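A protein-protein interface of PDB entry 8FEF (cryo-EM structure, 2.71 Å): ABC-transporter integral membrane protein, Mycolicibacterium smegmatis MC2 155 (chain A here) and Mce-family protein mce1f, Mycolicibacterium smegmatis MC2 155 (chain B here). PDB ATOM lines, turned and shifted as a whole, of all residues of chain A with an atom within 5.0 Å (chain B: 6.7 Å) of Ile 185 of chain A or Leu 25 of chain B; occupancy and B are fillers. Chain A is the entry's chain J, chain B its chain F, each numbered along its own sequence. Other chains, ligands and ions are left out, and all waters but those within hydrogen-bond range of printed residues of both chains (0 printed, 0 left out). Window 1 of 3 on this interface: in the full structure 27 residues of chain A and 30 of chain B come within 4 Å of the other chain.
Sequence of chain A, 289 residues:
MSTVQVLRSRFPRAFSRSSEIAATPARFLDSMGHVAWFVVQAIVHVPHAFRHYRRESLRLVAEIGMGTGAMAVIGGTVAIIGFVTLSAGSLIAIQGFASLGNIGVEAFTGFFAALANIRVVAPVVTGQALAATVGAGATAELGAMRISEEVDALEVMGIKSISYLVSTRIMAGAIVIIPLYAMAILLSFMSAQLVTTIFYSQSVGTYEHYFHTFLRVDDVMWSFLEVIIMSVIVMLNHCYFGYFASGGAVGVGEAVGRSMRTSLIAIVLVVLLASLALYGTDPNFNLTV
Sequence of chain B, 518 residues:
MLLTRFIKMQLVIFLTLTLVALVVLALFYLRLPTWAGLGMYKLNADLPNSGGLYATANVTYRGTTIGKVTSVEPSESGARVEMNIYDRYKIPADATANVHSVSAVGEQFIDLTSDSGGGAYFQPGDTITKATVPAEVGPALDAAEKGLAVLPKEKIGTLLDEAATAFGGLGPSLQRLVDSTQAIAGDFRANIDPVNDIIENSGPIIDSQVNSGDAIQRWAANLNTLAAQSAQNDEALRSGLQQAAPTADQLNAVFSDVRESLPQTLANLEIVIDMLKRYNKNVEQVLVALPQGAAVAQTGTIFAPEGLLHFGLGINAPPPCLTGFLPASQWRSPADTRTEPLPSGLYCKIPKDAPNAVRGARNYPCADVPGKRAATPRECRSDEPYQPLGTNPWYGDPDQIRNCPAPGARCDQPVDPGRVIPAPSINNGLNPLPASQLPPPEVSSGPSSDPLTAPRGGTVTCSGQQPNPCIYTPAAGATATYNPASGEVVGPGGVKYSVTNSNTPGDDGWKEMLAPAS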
ATOM      1  N   ILE A 118     -29.712  24.675  29.363  1.00  0.00           N
ATOM      2  CA  ILE A 118     -31.072  24.197  29.131  1.00  0.00           C
ATOM      3  C   ILE A 118     -31.989  25.339  28.709  1.00  0.00           C
ATOM      4  O   ILE A 118     -32.755  25.216  27.746  1.00  0.00           O
ATOM      5  CB  ILE A 118     -31.604  23.478  30.382  1.00  0.00           C
ATOM      6  CG1 ILE A 118     -30.846  22.169  30.599  1.00  0.00           C
ATOM      7  CG2 ILE A 118     -33.089  23.203  30.250  1.00  0.00           C
ATOM      8  CD1 ILE A 118     -30.989  21.195  29.455  1.00  0.00           C
ATOM      9  N   ALA A 122     -28.343  25.905  24.678  1.00  0.00           N
ATOM     10  CA  ALA A 122     -28.368  24.659  23.913  1.00  0.00           C
ATOM     11  C   ALA A 122     -29.528  24.568  22.927  1.00  0.00           C
ATOM     12  O   ALA A 122     -29.280  24.185  21.770  1.00  0.00           O
ATOM     13  CB  ALA A 122     -28.345  23.456  24.861  1.00  0.00           C
ATOM     14  N   TYR A 181     -30.688  16.118  19.370  1.00  0.00           N
ATOM     15  CA  TYR A 181     -30.715  17.025  20.511  1.00  0.00           C
ATOM     16  C   TYR A 181     -30.213  16.351  21.778  1.00  0.00           C
ATOM     17  O   TYR A 181     -29.648  17.025  22.646  1.00  0.00           O
ATOM     18  CB  TYR A 181     -32.118  17.582  20.728  1.00  0.00           C
ATOM     19  CG  TYR A 181     -32.158  18.641  21.803  1.00  0.00           C
ATOM     20  CD1 TYR A 181     -31.360  19.772  21.715  1.00  0.00           C
ATOM     21  CD2 TYR A 181     -32.989  18.512  22.905  1.00  0.00           C
ATOM     22  CE1 TYR A 181     -31.386  20.742  22.693  1.00  0.00           C
ATOM     23  CE2 TYR A 181     -33.025  19.479  23.888  1.00  0.00           C
ATOM     24  CZ  TYR A 181     -32.223  20.593  23.775  1.00  0.00           C
ATOM     25  OH  TYR A 181     -32.253  21.558  24.753  1.00  0.00           O
ATOM     26  N   ALA A 182     -30.400  15.037  21.909  1.00  0.00           N
ATOM     27  CA  ALA A 182     -29.810  14.324  23.038  1.00  0.00           C
ATOM     28  C   ALA A 182     -28.288  14.398  22.991  1.00  0.00           C
ATOM     29  O   ALA A 182     -27.637  14.672  24.007  1.00  0.00           O
ATOM     30  CB  ALA A 182     -30.281  12.872  23.047  1.00  0.00           C
ATOM     31  N   MET A 183     -27.705  14.174  21.810  1.00  0.00           N
ATOM     32  CA  MET A 183     -26.260  14.314  21.659  1.00  0.00           C
ATOM     33  C   MET A 183     -25.817  15.748  21.915  1.00  0.00           C
ATOM     34  O   MET A 183     -24.770  15.980  22.526  1.00  0.00           O
ATOM     35  CB  MET A 183     -25.821  13.868  20.265  1.00  0.00           C
ATOM     36  CG  MET A 183     -26.143  12.425  19.934  1.00  0.00           C
ATOM     37  SD  MET A 183     -25.883  12.047  18.191  1.00  0.00           S
ATOM     38  CE  MET A 183     -26.727  10.476  18.058  1.00  0.00           C
ATOM     39  N   ALA A 184     -26.599  16.722  21.446  1.00  0.00           N
ATOM     40  CA  ALA A 184     -26.258  18.125  21.653  1.00  0.00           C
ATOM     41  C   ALA A 184     -26.229  18.477  23.135  1.00  0.00           C
ATOM     42  O   ALA A 184     -25.285  19.115  23.616  1.00  0.00           O
ATOM     43  CB  ALA A 184     -27.257  19.009  20.910  1.00  0.00           C
ATOM     44  N   ILE A 185     -27.258  18.060  23.875  1.00  0.00           N
ATOM     45  CA  ILE A 185     -27.318  18.318  25.311  1.00  0.00           C
ATOM     46  C   ILE A 185     -26.172  17.619  26.029  1.00  0.00           C
ATOM     47  O   ILE A 185     -25.505  18.208  26.892  1.00  0.00           O
ATOM     48  CB  ILE A 185     -28.688  17.876  25.864  1.00  0.00           C
ATOM     49  CG1 ILE A 185     -29.765  18.889  25.493  1.00  0.00           C
ATOM     50  CG2 ILE A 185     -28.640  17.698  27.363  1.00  0.00           C
ATOM     51  CD1 ILE A 185     -29.568  20.234  26.141  1.00  0.00           C
ATOM     52  N   LEU A 186     -25.921  16.355  25.676  1.00  0.00           N
ATOM     53  CA  LEU A 186     -24.848  15.595  26.305  1.00  0.00           C
ATOM     54  C   LEU A 186     -23.498  16.265  26.089  1.00  0.00           C
ATOM     55  O   LEU A 186     -22.710  16.417  27.028  1.00  0.00           O
ATOM     56  CB  LEU A 186     -24.844  14.172  25.746  1.00  0.00           C
ATOM     57  CG  LEU A 186     -23.751  13.227  26.225  1.00  0.00           C
ATOM     58  CD1 LEU A 186     -23.898  13.013  27.708  1.00  0.00           C
ATOM     59  CD2 LEU A 186     -23.829  11.909  25.482  1.00  0.00           C
ATOM     60  N   LEU A 187     -23.226  16.699  24.857  1.00  0.00           N
ATOM     61  CA  LEU A 187     -21.935  17.302  24.546  1.00  0.00           C
ATOM     62  C   LEU A 187     -21.798  18.690  25.153  1.00  0.00           C
ATOM     63  O   LEU A 187     -20.699  19.070  25.567  1.00  0.00           O
ATOM     64  CB  LEU A 187     -21.725  17.340  23.036  1.00  0.00           C
ATOM     65  CG  LEU A 187     -21.535  15.948  22.434  1.00  0.00           C
ATOM     66  CD1 LEU A 187     -21.559  15.997  20.926  1.00  0.00           C
ATOM     67  CD2 LEU A 187     -20.239  15.331  22.927  1.00  0.00           C
ATOM     68  N   SER A 188     -22.887  19.460  25.224  1.00  0.00           N
ATOM     69  CA  SER A 188     -22.834  20.757  25.889  1.00  0.00           C
ATOM     70  C   SER A 188     -22.512  20.599  27.372  1.00  0.00           C
ATOM     71  O   SER A 188     -21.640  21.297  27.911  1.00  0.00           O
ATOM     72  CB  SER A 188     -24.159  21.491  25.695  1.00  0.00           C
ATOM     73  OG  SER A 188     -24.082  22.820  26.169  1.00  0.00           O
ATOM     74  N   PHE A 189     -23.202  19.671  28.045  1.00  0.00           N
ATOM     75  CA  PHE A 189     -22.916  19.406  29.453  1.00  0.00           C
ATOM     76  C   PHE A 189     -21.483  18.930  29.642  1.00  0.00           C
ATOM     77  O   PHE A 189     -20.785  19.376  30.562  1.00  0.00           O
ATOM     78  CB  PHE A 189     -23.890  18.367  30.009  1.00  0.00           C
ATOM     79  CG  PHE A 189     -25.292  18.875  30.197  1.00  0.00           C
ATOM     80  CD1 PHE A 189     -25.574  20.228  30.129  1.00  0.00           C
ATOM     81  CD2 PHE A 189     -26.325  17.993  30.456  1.00  0.00           C
ATOM     82  CE1 PHE A 189     -26.862  20.689  30.307  1.00  0.00           C
ATOM     83  CE2 PHE A 189     -27.612  18.450  30.636  1.00  0.00           C
ATOM     84  CZ  PHE A 189     -27.881  19.799  30.560  1.00  0.00           C
ATOM     85  N   MET A 190     -21.032  18.016  28.779  1.00  0.00           N
ATOM     86  CA  MET A 190     -19.682  17.477  28.892  1.00  0.00           C
ATOM     87  C   MET A 190     -18.635  18.563  28.697  1.00  0.00           C
ATOM     88  O   MET A 190     -17.644  18.613  29.432  1.00  0.00           O
ATOM     89  CB  MET A 190     -19.491  16.353  27.873  1.00  0.00           C
ATOM     90  CG  MET A 190     -18.141  15.670  27.935  1.00  0.00           C
ATOM     91  SD  MET A 190     -18.012  14.351  26.717  1.00  0.00           S
ATOM     92  CE  MET A 190     -19.438  13.359  27.149  1.00  0.00           C
ATOM     93  N   PHE A 224     -36.753  19.467  25.195  1.00  0.00           N
ATOM     94  CA  PHE A 224     -36.889  18.504  24.109  1.00  0.00           C
ATOM     95  C   PHE A 224     -38.141  18.773  23.287  1.00  0.00           C
ATOM     96  O   PHE A 224     -38.112  18.691  22.053  1.00  0.00           O
ATOM     97  CB  PHE A 224     -36.910  17.080  24.663  1.00  0.00           C
ATOM     98  CG  PHE A 224     -35.574  16.399  24.640  1.00  0.00           C
ATOM     99  CD1 PHE A 224     -34.698  16.524  25.704  1.00  0.00           C
ATOM    100  CD2 PHE A 224     -35.196  15.628  23.556  1.00  0.00           C
ATOM    101  CE1 PHE A 224     -33.468  15.896  25.683  1.00  0.00           C
ATOM    102  CE2 PHE A 224     -33.969  14.998  23.531  1.00  0.00           C
ATOM    103  CZ  PHE A 224     -33.104  15.132  24.597  1.00  0.00           C
ATOM    104  N   VAL B  20     -26.442   4.976  22.667  1.00  0.00           N
ATOM    105  CA  VAL B  20     -25.383   5.357  23.599  1.00  0.00           C
ATOM    106  C   VAL B  20     -25.676   6.722  24.209  1.00  0.00           C
ATOM    107  O   VAL B  20     -25.613   6.901  25.432  1.00  0.00           O
ATOM    108  CB  VAL B  20     -24.013   5.333  22.897  1.00  0.00           C
ATOM    109  CG1 VAL B  20     -22.959   5.998  23.765  1.00  0.00           C
ATOM    110  CG2 VAL B  20     -23.610   3.903  22.581  1.00  0.00           C
ATOM    111  N   ALA B  21     -26.024   7.699  23.365  1.00  0.00           N
ATOM    112  CA  ALA B  21     -26.293   9.045  23.857  1.00  0.00           C
ATOM    113  C   ALA B  21     -27.487   9.062  24.800  1.00  0.00           C
ATOM    114  O   ALA B  21     -27.437   9.696  25.860  1.00  0.00           O
ATOM    115  CB  ALA B  21     -26.525   9.996  22.684  1.00  0.00           C
ATOM    116  N   LEU B  22     -28.565   8.361  24.438  1.00  0.00           N
ATOM    117  CA  LEU B  22     -29.768   8.364  25.263  1.00  0.00           C
ATOM    118  C   LEU B  22     -29.503   7.732  26.623  1.00  0.00           C
ATOM    119  O   LEU B  22     -29.893   8.283  27.658  1.00  0.00           O
ATOM    120  CB  LEU B  22     -30.897   7.633  24.537  1.00  0.00           C
ATOM    121  CG  LEU B  22     -32.221   8.386  24.397  1.00  0.00           C
ATOM    122  CD1 LEU B  22     -32.008   9.701  23.681  1.00  0.00           C
ATOM    123  CD2 LEU B  22     -33.240   7.536  23.659  1.00  0.00           C
ATOM    124  N   VAL B  23     -28.821   6.583  26.643  1.00  0.00           N
ATOM    125  CA  VAL B  23     -28.552   5.909  27.911  1.00  0.00           C
ATOM    126  C   VAL B  23     -27.621   6.745  28.783  1.00  0.00           C
ATOM    127  O   VAL B  23     -27.857   6.899  29.989  1.00  0.00           O
ATOM    128  CB  VAL B  23     -27.990   4.499  27.659  1.00  0.00           C
ATOM    129  CG1 VAL B  23     -27.511   3.876  28.956  1.00  0.00           C
ATOM    130  CG2 VAL B  23     -29.052   3.620  27.022  1.00  0.00           C
ATOM    131  N   VAL B  24     -26.555   7.302  28.196  1.00  0.00           N
ATOM    132  CA  VAL B  24     -25.611   8.094  28.981  1.00  0.00           C
ATOM    133  C   VAL B  24     -26.290   9.335  29.547  1.00  0.00           C
ATOM    134  O   VAL B  24     -26.121   9.667  30.728  1.00  0.00           O
ATOM    135  CB  VAL B  24     -24.375   8.451  28.135  1.00  0.00           C
ATOM    136  CG1 VAL B  24     -23.531   9.497  28.839  1.00  0.00           C
ATOM    137  CG2 VAL B  24     -23.545   7.208  27.871  1.00  0.00           C
ATOM    138  N   LEU B  25     -27.082  10.029  28.725  1.00  0.00           N
ATOM    139  CA  LEU B  25     -27.781  11.218  29.196  1.00  0.00           C
ATOM    140  C   LEU B  25     -28.792  10.874  30.283  1.00  0.00           C
ATOM    141  O   LEU B  25     -28.933  11.612  31.264  1.00  0.00           O
ATOM    142  CB  LEU B  25     -28.470  11.917  28.023  1.00  0.00           C
ATOM    143  CG  LEU B  25     -29.183  13.234  28.325  1.00  0.00           C
ATOM    144  CD1 LEU B  25     -28.187  14.285  28.776  1.00  0.00           C
ATOM    145  CD2 LEU B  25     -29.957  13.713  27.113  1.00  0.00           C
ATOM    146  N   ALA B  26     -29.500   9.751  30.132  1.00  0.00           N
ATOM    147  CA  ALA B  26     -30.529   9.391  31.100  1.00  0.00           C
ATOM    148  C   ALA B  26     -29.925   8.968  32.431  1.00  0.00           C
ATOM    149  O   ALA B  26     -30.492   9.251  33.492  1.00  0.00           O
ATOM    150  CB  ALA B  26     -31.408   8.277  30.535  1.00  0.00           C
ATOM    151  N   LEU B  27     -28.776   8.293  32.405  1.00  0.00           N
ATOM    152  CA  LEU B  27     -28.217   7.743  33.636  1.00  0.00           C
ATOM    153  C   LEU B  27     -27.220   8.690  34.300  1.00  0.00           C
ATOM    154  O   LEU B  27     -27.398   9.068  35.461  1.00  0.00           O
ATOM    155  CB  LEU B  27     -27.556   6.389  33.350  1.00  0.00           C
ATOM    156  CG  LEU B  27     -28.476   5.277  32.847  1.00  0.00           C
ATOM    157  CD1 LEU B  27     -27.713   3.970  32.727  1.00  0.00           C
ATOM    158  CD2 LEU B  27     -29.680   5.118  33.758  1.00  0.00           C
ATOM    159  N   PHE B  28     -26.167   9.076  33.583  1.00  0.00           N
ATOM    160  CA  PHE B  28     -25.044   9.761  34.208  1.00  0.00           C
ATOM    161  C   PHE B  28     -25.215  11.271  34.304  1.00  0.00           C
ATOM    162  O   PHE B  28     -24.452  11.914  35.032  1.00  0.00           O
ATOM    163  CB  PHE B  28     -23.752   9.446  33.447  1.00  0.00           C
ATOM    164  CG  PHE B  28     -23.377   7.991  33.462  1.00  0.00           C
ATOM    165  CD1 PHE B  28     -23.916   7.111  32.537  1.00  0.00           C
ATOM    166  CD2 PHE B  28     -22.488   7.502  34.404  1.00  0.00           C
ATOM    167  CE1 PHE B  28     -23.575   5.773  32.550  1.00  0.00           C
ATOM    168  CE2 PHE B  28     -22.143   6.164  34.421  1.00  0.00           C
ATOM    169  CZ  PHE B  28     -22.688   5.300  33.492  1.00  0.00           C
ATOM    170  N   TYR B  29     -26.182  11.857  33.602  1.00  0.00           N
ATOM    171  CA  TYR B  29     -26.362  13.304  33.618  1.00  0.00           C
ATOM    172  C   TYR B  29     -27.721  13.732  34.147  1.00  0.00           C
ATOM    173  O   TYR B  29     -27.791  14.614  35.008  1.00  0.00           O
ATOM    174  CB  TYR B  29     -26.129  13.877  32.212  1.00  0.00           C
ATOM    175  CG  TYR B  29     -24.665  13.993  31.857  1.00  0.00           C
ATOM    176  CD1 TYR B  29     -23.977  12.925  31.299  1.00  0.00           C
ATOM    177  CD2 TYR B  29     -23.969  15.172  32.082  1.00  0.00           C
ATOM    178  CE1 TYR B  29     -22.639  13.028  30.978  1.00  0.00           C
ATOM    179  CE2 TYR B  29     -22.633  15.285  31.761  1.00  0.00           C
ATOM    180  CZ  TYR B  29     -21.973  14.211  31.209  1.00  0.00           C
ATOM    181  OH  TYR B  29     -20.641  14.319  30.890  1.00  0.00           O
ATOM    182  N   LEU B  30     -28.807  13.139  33.655  1.00  0.00           N
ATOM    183  CA  LEU B  30     -30.138  13.514  34.114  1.00  0.00           C
ATOM    184  C   LEU B  30     -30.578  12.755  35.356  1.00  0.00           C
ATOM    185  O   LEU B  30     -31.427  13.262  36.098  1.00  0.00           O
ATOM    186  CB  LEU B  30     -31.169  13.291  33.004  1.00  0.00           C
ATOM    187  CG  LEU B  30     -30.996  14.116  31.730  1.00  0.00           C
ATOM    188  CD1 LEU B  30     -32.165  13.889  30.789  1.00  0.00           C
ATOM    189  CD2 LEU B  30     -30.848  15.584  32.069  1.00  0.00           C
ATOM    190  N   ARG B  31     -30.018  11.568  35.596  1.00  0.00           N
ATOM    191  CA  ARG B  31     -30.392  10.704  36.717  1.00  0.00           C
ATOM    192  C   ARG B  31     -31.893  10.410  36.710  1.00  0.00           C
ATOM    193  O   ARG B  31     -32.623  10.716  37.654  1.00  0.00           O
ATOM    194  CB  ARG B  31     -29.949  11.311  38.054  1.00  0.00           C
ATOM    195  CG  ARG B  31     -28.446  11.448  38.202  1.00  0.00           C
ATOM    196  CD  ARG B  31     -28.081  11.974  39.576  1.00  0.00           C
ATOM    197  NE  ARG B  31     -26.637  12.031  39.774  1.00  0.00           N
ATOM    198  CZ  ARG B  31     -26.051  12.390  40.906  1.00  0.00           C
ATOM    199  NH1 ARG B  31     -26.758  12.733  41.972  1.00  0.00           N
ATOM    200  NH2 ARG B  31     -24.724  12.403  40.975  1.00  0.00           N
ATOM    201  N   LEU B  32     -32.343   9.821  35.602  1.00  0.00           N
ATOM    202  CA  LEU B  32     -33.747   9.437  35.483  1.00  0.00           C
ATOM    203  C   LEU B  32     -34.214   8.436  36.537  1.00  0.00           C
ATOM    204  O   LEU B  32     -35.357   8.581  37.003  1.00  0.00           O
ATOM    205  CB  LEU B  32     -34.027   8.905  34.071  1.00  0.00           C
ATOM    206  CG  LEU B  32     -34.210   9.958  32.979  1.00  0.00           C
ATOM    207  CD1 LEU B  32     -34.725   9.322  31.702  1.00  0.00           C
ATOM    208  CD2 LEU B  32     -35.162  11.033  33.454  1.00  0.00           C
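The backbone carbonyl oxygen (O) of Leu 25 of chain B sits at hydrogen-bond distance from the backbone NH (N) of Leu 30 of chain B, at 2.8 Å.
CB of Ala 182 of chain A touches CD1 of Leu 22 of chain B (3.7 Å).
CD2 of Leu 25 of chain B touches O of Ala 182 of chain A (3.99 Å).
CB of Ala 21 of chain B touches CG of Met 183 of chain A (3.7 Å).
CG2 of Ile 185 of chain A touches CD1 of Leu 25 of chain B, at 3.7 Å.
Leu 186 of chain A touches Val 24 of chain B.
Tyr 29 of chain B touches Leu 186 of chain A (CE1 to CD1, 3.5 Å).
Phe 189 of chain A touches Tyr 29 of chain B.
Met 190 of chain A touches Tyr 29 of chain B (CB to OH, 3.8 Å).
Ile 185 of chain A touches just one residue of chain B: Leu 25 (3.7 Å).
Printed residues of chain A within 4 Å of Leu 25 of chain B: Ala 182 and Ile 185.
Of the printed residues of chain A, Leu 22 of chain B touches Ala 182 (3.7 Å).
Of the printed residues of chain B, Leu 186 of chain A touches Val 24 and Tyr 29.
Of the printed residues of chain B, Ala 182 of chain A touches Leu 22 (3.7 Å) and Leu 25 (3.99 Å).
The nearest residue of chain B that does not touch Ile 185 of chain A is Leu 30 of chain B (5.6 Å).
The nearest printed residue of chain A that does not touch Leu 25 of chain B is Phe 224 of chain A (4.3 Å).
Of the 13 printed residues of chain A, 6 touch a printed residue of chain B.
Printed residues of chain A that touch a printed residue of chain B: Ala 182, Met 183, Ile 185, Leu 186, Phe 189 and Met 190.
Hydrophobic or aromatic side chains of chain B within 4 Å of the printed part of chain A: Ala 21, Leu 22, Val 24, Leu 25 and Tyr 29.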
